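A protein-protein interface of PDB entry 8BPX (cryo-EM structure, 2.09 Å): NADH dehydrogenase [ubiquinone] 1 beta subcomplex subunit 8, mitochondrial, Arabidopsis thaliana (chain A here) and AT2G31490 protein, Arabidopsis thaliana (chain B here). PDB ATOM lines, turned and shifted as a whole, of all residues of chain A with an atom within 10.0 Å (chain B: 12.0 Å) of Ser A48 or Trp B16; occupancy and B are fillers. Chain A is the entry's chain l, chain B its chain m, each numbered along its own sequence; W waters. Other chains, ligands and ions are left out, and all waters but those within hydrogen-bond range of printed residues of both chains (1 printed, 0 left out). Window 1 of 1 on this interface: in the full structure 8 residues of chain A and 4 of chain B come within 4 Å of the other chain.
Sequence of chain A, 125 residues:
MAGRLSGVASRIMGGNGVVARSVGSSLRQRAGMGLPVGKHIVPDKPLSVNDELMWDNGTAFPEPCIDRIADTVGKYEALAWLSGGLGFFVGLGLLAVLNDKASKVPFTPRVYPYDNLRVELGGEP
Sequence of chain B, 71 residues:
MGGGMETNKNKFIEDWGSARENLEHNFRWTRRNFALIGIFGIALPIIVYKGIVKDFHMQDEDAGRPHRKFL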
ATOM      1  N   PRO A  43     -10.350  -8.834  -8.518  1.00  0.00           N
ATOM      2  CA  PRO A  43     -10.023  -8.931  -9.947  1.00  0.00           C
ATOM      3  C   PRO A  43      -8.946  -7.941 -10.368  1.00  0.00           C
ATOM      4  O   PRO A  43      -8.923  -6.792  -9.922  1.00  0.00           O
ATOM      5  CB  PRO A  43     -11.358  -8.631 -10.634  1.00  0.00           C
ATOM      6  CG  PRO A  43     -12.394  -8.976  -9.624  1.00  0.00           C
ATOM      7  CD  PRO A  43     -11.796  -8.674  -8.284  1.00  0.00           C
ATOM      8  N   LYS A  45      -8.127  -8.176 -13.950  1.00  0.00           N
ATOM      9  CA  LYS A  45      -8.406  -8.178 -15.376  1.00  0.00           C
ATOM     10  C   LYS A  45      -9.873  -7.850 -15.582  1.00  0.00           C
ATOM     11  O   LYS A  45     -10.690  -8.040 -14.675  1.00  0.00           O
ATOM     12  CB  LYS A  45      -8.089  -9.542 -16.007  1.00  0.00           C
ATOM     13  CG  LYS A  45      -6.661 -10.012 -15.827  1.00  0.00           C
ATOM     14  CD  LYS A  45      -6.412 -11.437 -16.346  1.00  0.00           C
ATOM     15  CE  LYS A  45      -7.580 -12.421 -16.160  1.00  0.00           C
ATOM     16  NZ  LYS A  45      -8.360 -12.295 -14.891  1.00  0.00           N
ATOM     17  N   PRO A  46     -10.243  -7.332 -16.753  1.00  0.00           N
ATOM     18  CA  PRO A  46     -11.663  -7.074 -17.019  1.00  0.00           C
ATOM     19  C   PRO A  46     -12.485  -8.352 -16.929  1.00  0.00           C
ATOM     20  O   PRO A  46     -12.098  -9.401 -17.445  1.00  0.00           O
ATOM     21  CB  PRO A  46     -11.659  -6.497 -18.438  1.00  0.00           C
ATOM     22  CG  PRO A  46     -10.288  -5.925 -18.599  1.00  0.00           C
ATOM     23  CD  PRO A  46      -9.379  -6.827 -17.832  1.00  0.00           C
ATOM     24  N   LEU A  47     -13.620  -8.256 -16.246  1.00  0.00           N
ATOM     25  CA  LEU A  47     -14.515  -9.392 -16.127  1.00  0.00           C
ATOM     26  C   LEU A  47     -15.260  -9.619 -17.436  1.00  0.00           C
ATOM     27  O   LEU A  47     -15.509  -8.689 -18.207  1.00  0.00           O
ATOM     28  CB  LEU A  47     -15.508  -9.173 -14.990  1.00  0.00           C
ATOM     29  CG  LEU A  47     -14.889  -8.833 -13.636  1.00  0.00           C
ATOM     30  CD1 LEU A  47     -15.960  -8.429 -12.646  1.00  0.00           C
ATOM     31  CD2 LEU A  47     -14.078  -9.998 -13.120  1.00  0.00           C
ATOM     32  N   SER A  48     -15.601 -10.879 -17.687  1.00  0.00           N
ATOM     33  CA  SER A  48     -16.399 -11.227 -18.848  1.00  0.00           C
ATOM     34  C   SER A  48     -17.869 -10.902 -18.596  1.00  0.00           C
ATOM     35  O   SER A  48     -18.280 -10.574 -17.481  1.00  0.00           O
ATOM     36  CB  SER A  48     -16.234 -12.705 -19.193  1.00  0.00           C
ATOM     37  OG  SER A  48     -16.141 -13.499 -18.025  1.00  0.00           O
ATOM     38  N   VAL A  49     -18.667 -11.000 -19.659  1.00  0.00           N
ATOM     39  CA  VAL A  49     -20.096 -10.733 -19.548  1.00  0.00           C
ATOM     40  C   VAL A  49     -20.783 -11.791 -18.690  1.00  0.00           C
ATOM     41  O   VAL A  49     -21.635 -11.470 -17.856  1.00  0.00           O
ATOM     42  CB  VAL A  49     -20.732 -10.630 -20.947  1.00  0.00           C
ATOM     43  CG1 VAL A  49     -20.237  -9.378 -21.652  1.00  0.00           C
ATOM     44  CG2 VAL A  49     -20.408 -11.857 -21.776  1.00  0.00           C
ATOM     45  N   ASN A  50     -20.437 -13.059 -18.885  1.00  0.00           N
ATOM     46  CA  ASN A  50     -21.038 -14.144 -18.116  1.00  0.00           C
ATOM     47  C   ASN A  50     -20.072 -14.602 -17.026  1.00  0.00           C
ATOM     48  O   ASN A  50     -19.479 -15.679 -17.075  1.00  0.00           O
ATOM     49  CB  ASN A  50     -21.440 -15.288 -19.041  1.00  0.00           C
ATOM     50  CG  ASN A  50     -22.655 -14.954 -19.878  1.00  0.00           C
ATOM     51  OD1 ASN A  50     -22.843 -13.811 -20.294  1.00  0.00           O
ATOM     52  ND2 ASN A  50     -23.496 -15.951 -20.119  1.00  0.00           N
ATOM     53  N   ASP A  51     -19.934 -13.744 -16.020  1.00  0.00           N
ATOM     54  CA  ASP A  51     -19.074 -14.006 -14.877  1.00  0.00           C
ATOM     55  C   ASP A  51     -19.861 -14.206 -13.591  1.00  0.00           C
ATOM     56  O   ASP A  51     -19.303 -14.709 -12.613  1.00  0.00           O
ATOM     57  CB  ASP A  51     -18.076 -12.852 -14.698  1.00  0.00           C
ATOM     58  CG  ASP A  51     -16.934 -13.202 -13.773  1.00  0.00           C
ATOM     59  OD1 ASP A  51     -16.667 -14.408 -13.573  1.00  0.00           O
ATOM     60  OD2 ASP A  51     -16.298 -12.269 -13.245  1.00  0.00           O
ATOM     61  N   GLU A  52     -21.143 -13.836 -13.579  1.00  0.00           N
ATOM     62  CA  GLU A  52     -21.985 -14.039 -12.408  1.00  0.00           C
ATOM     63  C   GLU A  52     -22.213 -15.511 -12.104  1.00  0.00           C
ATOM     64  O   GLU A  52     -22.594 -15.843 -10.976  1.00  0.00           O
ATOM     65  CB  GLU A  52     -23.334 -13.360 -12.614  1.00  0.00           C
ATOM     66  CG  GLU A  52     -24.037 -13.822 -13.875  1.00  0.00           C
ATOM     67  CD  GLU A  52     -24.097 -12.752 -14.929  1.00  0.00           C
ATOM     68  OE1 GLU A  52     -23.023 -12.340 -15.420  1.00  0.00           O
ATOM     69  OE2 GLU A  52     -25.216 -12.328 -15.276  1.00  0.00           O
ATOM     70  N   LEU A  53     -22.006 -16.395 -13.081  1.00  0.00           N
ATOM     71  CA  LEU A  53     -22.336 -17.805 -12.935  1.00  0.00           C
ATOM     72  C   LEU A  53     -21.142 -18.740 -13.058  1.00  0.00           C
ATOM     73  O   LEU A  53     -21.322 -19.958 -12.942  1.00  0.00           O
ATOM     74  CB  LEU A  53     -23.404 -18.209 -13.965  1.00  0.00           C
ATOM     75  CG  LEU A  53     -23.310 -17.727 -15.417  1.00  0.00           C
ATOM     76  CD1 LEU A  53     -22.199 -18.421 -16.187  1.00  0.00           C
ATOM     77  CD2 LEU A  53     -24.637 -17.908 -16.128  1.00  0.00           C
ATOM     78  N   MET A  54     -19.942 -18.225 -13.291  1.00  0.00           N
ATOM     79  CA  MET A  54     -18.783 -19.085 -13.498  1.00  0.00           C
ATOM     80  C   MET A  54     -17.998 -19.277 -12.205  1.00  0.00           C
ATOM     81  O   MET A  54     -17.617 -20.395 -11.861  1.00  0.00           O
ATOM     82  CB  MET A  54     -17.875 -18.511 -14.587  1.00  0.00           C
ATOM     83  CG  MET A  54     -17.961 -19.243 -15.919  1.00  0.00           C
ATOM     84  SD  MET A  54     -17.693 -21.019 -15.766  1.00  0.00           S
ATOM     85  CE  MET A  54     -15.909 -21.106 -15.899  1.00  0.00           C
ATOM     86  N   LYS B   9     -14.343   0.648  -4.056  1.00  0.00           N
ATOM     87  CA  LYS B   9     -14.670   0.290  -5.428  1.00  0.00           C
ATOM     88  C   LYS B   9     -13.508  -0.437  -6.091  1.00  0.00           C
ATOM     89  O   LYS B   9     -12.339  -0.132  -5.847  1.00  0.00           O
ATOM     90  CB  LYS B   9     -15.010   1.547  -6.228  1.00  0.00           C
ATOM     91  CG  LYS B   9     -16.466   1.739  -6.569  1.00  0.00           C
ATOM     92  CD  LYS B   9     -17.403   1.411  -5.431  1.00  0.00           C
ATOM     93  CE  LYS B   9     -18.737   2.108  -5.664  1.00  0.00           C
ATOM     94  NZ  LYS B   9     -19.659   2.080  -4.506  1.00  0.00           N
ATOM     95  N   ASN B  10     -13.842  -1.414  -6.923  1.00  0.00           N
ATOM     96  CA  ASN B  10     -12.893  -2.066  -7.813  1.00  0.00           C
ATOM     97  C   ASN B  10     -13.207  -1.628  -9.238  1.00  0.00           C
ATOM     98  O   ASN B  10     -14.358  -1.717  -9.675  1.00  0.00           O
ATOM     99  CB  ASN B  10     -12.967  -3.588  -7.687  1.00  0.00           C
ATOM    100  CG  ASN B  10     -12.143  -4.304  -8.738  1.00  0.00           C
ATOM    101  OD1 ASN B  10     -12.613  -4.565  -9.842  1.00  0.00           O
ATOM    102  ND2 ASN B  10     -10.909  -4.641  -8.391  1.00  0.00           N
ATOM    103  N   LYS B  11     -12.184  -1.165  -9.956  1.00  0.00           N
ATOM    104  CA  LYS B  11     -12.409  -0.544 -11.259  1.00  0.00           C
ATOM    105  C   LYS B  11     -12.997  -1.532 -12.259  1.00  0.00           C
ATOM    106  O   LYS B  11     -13.860  -1.170 -13.065  1.00  0.00           O
ATOM    107  CB  LYS B  11     -11.102   0.058 -11.781  1.00  0.00           C
ATOM    108  CG  LYS B  11     -10.919  -0.007 -13.285  1.00  0.00           C
ATOM    109  CD  LYS B  11      -9.785   0.908 -13.737  1.00  0.00           C
ATOM    110  CE  LYS B  11      -9.090   0.370 -14.974  1.00  0.00           C
ATOM    111  NZ  LYS B  11      -8.539  -0.992 -14.749  1.00  0.00           N
ATOM    112  N   PHE B  12     -12.550  -2.785 -12.221  1.00  0.00           N
ATOM    113  CA  PHE B  12     -13.052  -3.778 -13.164  1.00  0.00           C
ATOM    114  C   PHE B  12     -14.497  -4.162 -12.863  1.00  0.00           C
ATOM    115  O   PHE B  12     -15.291  -4.372 -13.784  1.00  0.00           O
ATOM    116  CB  PHE B  12     -12.146  -5.002 -13.146  1.00  0.00           C
ATOM    117  CG  PHE B  12     -10.712  -4.683 -13.432  1.00  0.00           C
ATOM    118  CD1 PHE B  12     -10.255  -4.622 -14.735  1.00  0.00           C
ATOM    119  CD2 PHE B  12      -9.826  -4.418 -12.399  1.00  0.00           C
ATOM    120  CE1 PHE B  12      -8.936  -4.327 -15.006  1.00  0.00           C
ATOM    121  CE2 PHE B  12      -8.506  -4.119 -12.667  1.00  0.00           C
ATOM    122  CZ  PHE B  12      -8.064  -4.070 -13.971  1.00  0.00           C
ATOM    123  N   ILE B  13     -14.856  -4.249 -11.580  1.00  0.00           N
ATOM    124  CA  ILE B  13     -16.233  -4.556 -11.203  1.00  0.00           C
ATOM    125  C   ILE B  13     -17.172  -3.439 -11.646  1.00  0.00           C
ATOM    126  O   ILE B  13     -18.258  -3.691 -12.181  1.00  0.00           O
ATOM    127  CB  ILE B  13     -16.314  -4.812  -9.687  1.00  0.00           C
ATOM    128  CG1 ILE B  13     -15.575  -6.102  -9.334  1.00  0.00           C
ATOM    129  CG2 ILE B  13     -17.754  -4.895  -9.227  1.00  0.00           C
ATOM    130  CD1 ILE B  13     -15.402  -6.308  -7.851  1.00  0.00           C
ATOM    131  N   GLU B  14     -16.758  -2.186 -11.450  1.00  0.00           N
ATOM    132  CA  GLU B  14     -17.571  -1.064 -11.909  1.00  0.00           C
ATOM    133  C   GLU B  14     -17.640  -0.995 -13.430  1.00  0.00           C
ATOM    134  O   GLU B  14     -18.688  -0.650 -13.984  1.00  0.00           O
ATOM    135  CB  GLU B  14     -17.046   0.241 -11.319  1.00  0.00           C
ATOM    136  CG  GLU B  14     -16.987   0.194  -9.816  1.00  0.00           C
ATOM    137  CD  GLU B  14     -18.351   0.418  -9.193  1.00  0.00           C
ATOM    138  OE1 GLU B  14     -18.557   0.002  -8.038  1.00  0.00           O
ATOM    139  OE2 GLU B  14     -19.224   1.008  -9.863  1.00  0.00           O
ATOM    140  N   ASP B  15     -16.542  -1.316 -14.120  1.00  0.00           N
ATOM    141  CA  ASP B  15     -16.586  -1.378 -15.579  1.00  0.00           C
ATOM    142  C   ASP B  15     -17.578  -2.430 -16.051  1.00  0.00           C
ATOM    143  O   ASP B  15     -18.360  -2.188 -16.974  1.00  0.00           O
ATOM    144  CB  ASP B  15     -15.196  -1.677 -16.140  1.00  0.00           C
ATOM    145  CG  ASP B  15     -14.281  -0.483 -16.085  1.00  0.00           C
ATOM    146  OD1 ASP B  15     -13.049  -0.672 -16.050  1.00  0.00           O
ATOM    147  OD2 ASP B  15     -14.798   0.652 -16.065  1.00  0.00           O
ATOM    148  N   TRP B  16     -17.558  -3.603 -15.417  1.00  0.00           N
ATOM    149  CA  TRP B  16     -18.505  -4.667 -15.727  1.00  0.00           C
ATOM    150  C   TRP B  16     -19.946  -4.209 -15.508  1.00  0.00           C
ATOM    151  O   TRP B  16     -20.811  -4.397 -16.376  1.00  0.00           O
ATOM    152  CB  TRP B  16     -18.157  -5.869 -14.853  1.00  0.00           C
ATOM    153  CG  TRP B  16     -18.982  -7.097 -14.979  1.00  0.00           C
ATOM    154  CD1 TRP B  16     -19.143  -7.874 -16.085  1.00  0.00           C
ATOM    155  CD2 TRP B  16     -19.737  -7.713 -13.938  1.00  0.00           C
ATOM    156  NE1 TRP B  16     -19.958  -8.939 -15.796  1.00  0.00           N
ATOM    157  CE2 TRP B  16     -20.337  -8.862 -14.483  1.00  0.00           C
ATOM    158  CE3 TRP B  16     -19.967  -7.401 -12.594  1.00  0.00           C
ATOM    159  CZ2 TRP B  16     -21.158  -9.700 -13.732  1.00  0.00           C
ATOM    160  CZ3 TRP B  16     -20.776  -8.233 -11.852  1.00  0.00           C
ATOM    161  CH2 TRP B  16     -21.361  -9.370 -12.422  1.00  0.00           C
ATOM    162  N   GLY B  17     -20.210  -3.564 -14.370  1.00  0.00           N
ATOM    163  CA  GLY B  17     -21.554  -3.077 -14.096  1.00  0.00           C
ATOM    164  C   GLY B  17     -22.028  -2.029 -15.088  1.00  0.00           C
ATOM    165  O   GLY B  17     -23.155  -2.100 -15.591  1.00  0.00           O
ATOM    166  N   SER B  18     -21.175  -1.048 -15.392  1.00  0.00           N
ATOM    167  CA  SER B  18     -21.562   0.000 -16.332  1.00  0.00           C
ATOM    168  C   SER B  18     -21.738  -0.546 -17.742  1.00  0.00           C
ATOM    169  O   SER B  18     -22.613  -0.081 -18.477  1.00  0.00           O
ATOM    170  CB  SER B  18     -20.541   1.138 -16.317  1.00  0.00           C
ATOM    171  OG  SER B  18     -19.214   0.652 -16.340  1.00  0.00           O
ATOM    172  N   ALA B  19     -20.927  -1.531 -18.137  1.00  0.00           N
ATOM    173  CA  ALA B  19     -21.144  -2.190 -19.419  1.00  0.00           C
ATOM    174  C   ALA B  19     -22.502  -2.876 -19.449  1.00  0.00           C
ATOM    175  O   ALA B  19     -23.202  -2.838 -20.467  1.00  0.00           O
ATOM    176  CB  ALA B  19     -20.029  -3.198 -19.692  1.00  0.00           C
ATOM    177  N   ARG B  20     -22.900  -3.457 -18.315  1.00  0.00           N
ATOM    178  CA  ARG B  20     -24.241  -4.094 -18.220  1.00  0.00           C
ATOM    179  C   ARG B  20     -25.321  -3.019 -18.391  1.00  0.00           C
ATOM    180  O   ARG B  20     -26.320  -3.301 -19.084  1.00  0.00           O
ATOM    181  CB  ARG B  20     -24.389  -4.825 -16.883  1.00  0.00           C
ATOM    182  CG  ARG B  20     -25.714  -5.552 -16.707  1.00  0.00           C
ATOM    183  CD  ARG B  20     -25.989  -6.567 -17.801  1.00  0.00           C
ATOM    184  NE  ARG B  20     -24.940  -7.573 -17.921  1.00  0.00           N
ATOM    185  CZ  ARG B  20     -24.860  -8.687 -17.200  1.00  0.00           C
ATOM    186  NH1 ARG B  20     -25.771  -8.958 -16.282  1.00  0.00           N
ATOM    187  NH2 ARG B  20     -23.859  -9.524 -17.398  1.00  0.00           N
ATOM    188  N   GLU B  21     -25.123  -1.833 -17.802  1.00  0.00           N
ATOM    189  CA  GLU B  21     -26.154  -0.799 -17.866  1.00  0.00           C
ATOM    190  C   GLU B  21     -26.287  -0.136 -19.236  1.00  0.00           C
ATOM    191  O   GLU B  21     -27.263   0.587 -19.453  1.00  0.00           O
ATOM    192  CB  GLU B  21     -25.898   0.295 -16.822  1.00  0.00           C
ATOM    193  CG  GLU B  21     -25.785  -0.195 -15.402  1.00  0.00           C
ATOM    194  CD  GLU B  21     -24.690   0.510 -14.626  1.00  0.00           C
ATOM    195  OE1 GLU B  21     -24.367   0.055 -13.512  1.00  0.00           O
ATOM    196  OE2 GLU B  21     -24.155   1.521 -15.124  1.00  0.00           O
ATOM    197  N   ASN B  22     -25.358  -0.353 -20.160  1.00  0.00           N
ATOM    198  CA  ASN B  22     -25.348   0.368 -21.426  1.00  0.00           C
ATOM    199  C   ASN B  22     -25.322  -0.580 -22.619  1.00  0.00           C
ATOM    200  O   ASN B  22     -24.687  -0.312 -23.638  1.00  0.00           O
ATOM    201  CB  ASN B  22     -24.174   1.340 -21.475  1.00  0.00           C
ATOM    202  CG  ASN B  22     -24.220   2.352 -20.352  1.00  0.00           C
ATOM    203  OD1 ASN B  22     -23.298   2.451 -19.548  1.00  0.00           O
ATOM    204  ND2 ASN B  22     -25.309   3.100 -20.284  1.00  0.00           N
ATOM    205  N   LEU B  23     -26.049  -1.692 -22.508  1.00  0.00           N
ATOM    206  CA  LEU B  23     -26.010  -2.716 -23.545  1.00  0.00           C
ATOM    207  C   LEU B  23     -26.646  -2.245 -24.849  1.00  0.00           C
ATOM    208  O   LEU B  23     -26.242  -2.693 -25.925  1.00  0.00           O
ATOM    209  CB  LEU B  23     -26.702  -3.980 -23.037  1.00  0.00           C
ATOM    210  CG  LEU B  23     -26.126  -5.325 -23.467  1.00  0.00           C
ATOM    211  CD1 LEU B  23     -24.616  -5.339 -23.296  1.00  0.00           C
ATOM    212  CD2 LEU B  23     -26.771  -6.449 -22.664  1.00  0.00           C
ATOM    213  N   GLU B  24     -27.625  -1.340 -24.777  1.00  0.00           N
ATOM    214  CA  GLU B  24     -28.365  -0.940 -25.971  1.00  0.00           C
ATOM    215  C   GLU B  24     -27.475  -0.270 -27.010  1.00  0.00           C
ATOM    216  O   GLU B  24     -27.807  -0.292 -28.198  1.00  0.00           O
ATOM    217  CB  GLU B  24     -29.520  -0.006 -25.596  1.00  0.00           C
ATOM    218  CG  GLU B  24     -29.116   1.279 -24.866  1.00  0.00           C
ATOM    219  CD  GLU B  24     -28.781   1.074 -23.404  1.00  0.00           C
ATOM    220  OE1 GLU B  24     -28.801  -0.081 -22.930  1.00  0.00           O
ATOM    221  OE2 GLU B  24     -28.498   2.076 -22.718  1.00  0.00           O
ATOM    222  N   HIS B  25     -26.352   0.310 -26.594  1.00  0.00           N
ATOM    223  CA  HIS B  25     -25.413   0.911 -27.532  1.00  0.00           C
ATOM    224  C   HIS B  25     -24.654  -0.120 -28.349  1.00  0.00           C
ATOM    225  O   HIS B  25     -23.976   0.251 -29.309  1.00  0.00           O
ATOM    226  CB  HIS B  25     -24.426   1.802 -26.779  1.00  0.00           C
ATOM    227  CG  HIS B  25     -25.074   2.944 -26.069  1.00  0.00           C
ATOM    228  ND1 HIS B  25     -24.992   3.114 -24.706  1.00  0.00           N
ATOM    229  CD2 HIS B  25     -25.824   3.970 -26.533  1.00  0.00           C
ATOM    230  CE1 HIS B  25     -25.666   4.194 -24.359  1.00  0.00           C
ATOM    231  NE2 HIS B  25     -26.180   4.733 -25.448  1.00  0.00           N
ATOM    232  N   ASN B  26     -24.761  -1.400 -28.005  1.00  0.00           N
ATOM    233  CA  ASN B  26     -24.012  -2.447 -28.675  1.00  0.00           C
ATOM    234  C   ASN B  26     -24.831  -3.195 -29.716  1.00  0.00           C
ATOM    235  O   ASN B  26     -24.251  -3.930 -30.521  1.00  0.00           O
ATOM    236  CB  ASN B  26     -23.483  -3.441 -27.641  1.00  0.00           C
ATOM    237  CG  ASN B  26     -22.417  -2.839 -26.763  1.00  0.00           C
ATOM    238  OD1 ASN B  26     -21.842  -1.802 -27.090  1.00  0.00           O
ATOM    239  ND2 ASN B  26     -22.145  -3.484 -25.634  1.00  0.00           N
HETATM  240  O   HOH W   1     -14.440  -5.435 -16.045  1.00  0.00           O
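ND2 of Asn B10 sits at hydrogen-bond distance from O of Pro A43, 3.3 Å away. The backbone carbonyl oxygen (O) of Ser A48 is in hydrogen-bond range of the indole nitrogen (NE1) of Trp B16. O of Val A49 is in hydrogen-bond range of NH2 of Arg B20, 3.0 Å away. The side-chain carboxylate (OE1) of Glu A52 lies within salt-bridge range of the guanidinium group (NH2) of Arg B20.
OD1 of Asn B10 sits at hydrogen-bond distance from N of Phe B12. N of Ile B13 is in hydrogen-bond range of OD1 of Asn B10 (2.9 Å).
Of chain B, only Trp B16 (2.9 Å) comes within 4 Å of Ser A48. Printed residues of chain A within 4 Å of Trp B16: Ser A48, Val A49 and Glu A52. Pro A46 touches just one residue of chain B: Phe B12 (3.4 Å). Val A49 touches just these residues of chain B: Trp B16 and Arg B20. No residue of chain B comes within 4 Å of Asn A50. No residue of chain B comes within 4 Å of Asp A51. Glu A52 touches two residues of chain B. Asp B15 touches none of the printed residues of chain A. No residue of chain A comes within 4 Å of Gly B17. Of the printed residues of chain A, Asn B10 touches Pro A43. Of the printed residues of chain B, Lys A45 touches Phe B12.
Of the 18 printed residues of chain B, 4 touch a printed residue of chain A. Hydrophobic or aromatic side chains of chain B that line the printed part of chain A: Phe B12 and Trp B16. Of the 11 printed residues of chain A, 6 touch a printed residue of chain B. Printed residues of chain A that touch a printed residue of chain B: Pro A43, Lys A45, Pro A46, Ser A48, Val A49 and Glu A52. Hydrophobic or aromatic side chains of chain A within 4 Å of the printed part of chain B: Pro A46. Among the printed residues, Asp or Glu carboxylates within 4 Å of a Lys or Arg side-chain nitrogen of the other chain: Glu A52 with Arg B20 (3.5 Å).
Among the printed residues, pairs that only touch across the chains: Pro A43 with Phe B12 (3.5 Å), Lys A45 with Phe B12 (3.4 Å), Pro A46 with Phe B12 (3.4 Å), Val A49 with Trp B16 (3.7 Å) and Glu A52 with Trp B16 (3.6 Å).
Water W1 bridges the backbone carbonyl oxygen (O) of Phe B12 (2.6 Å) and the backbone NH (N) of Leu A47 (2.9 Å).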
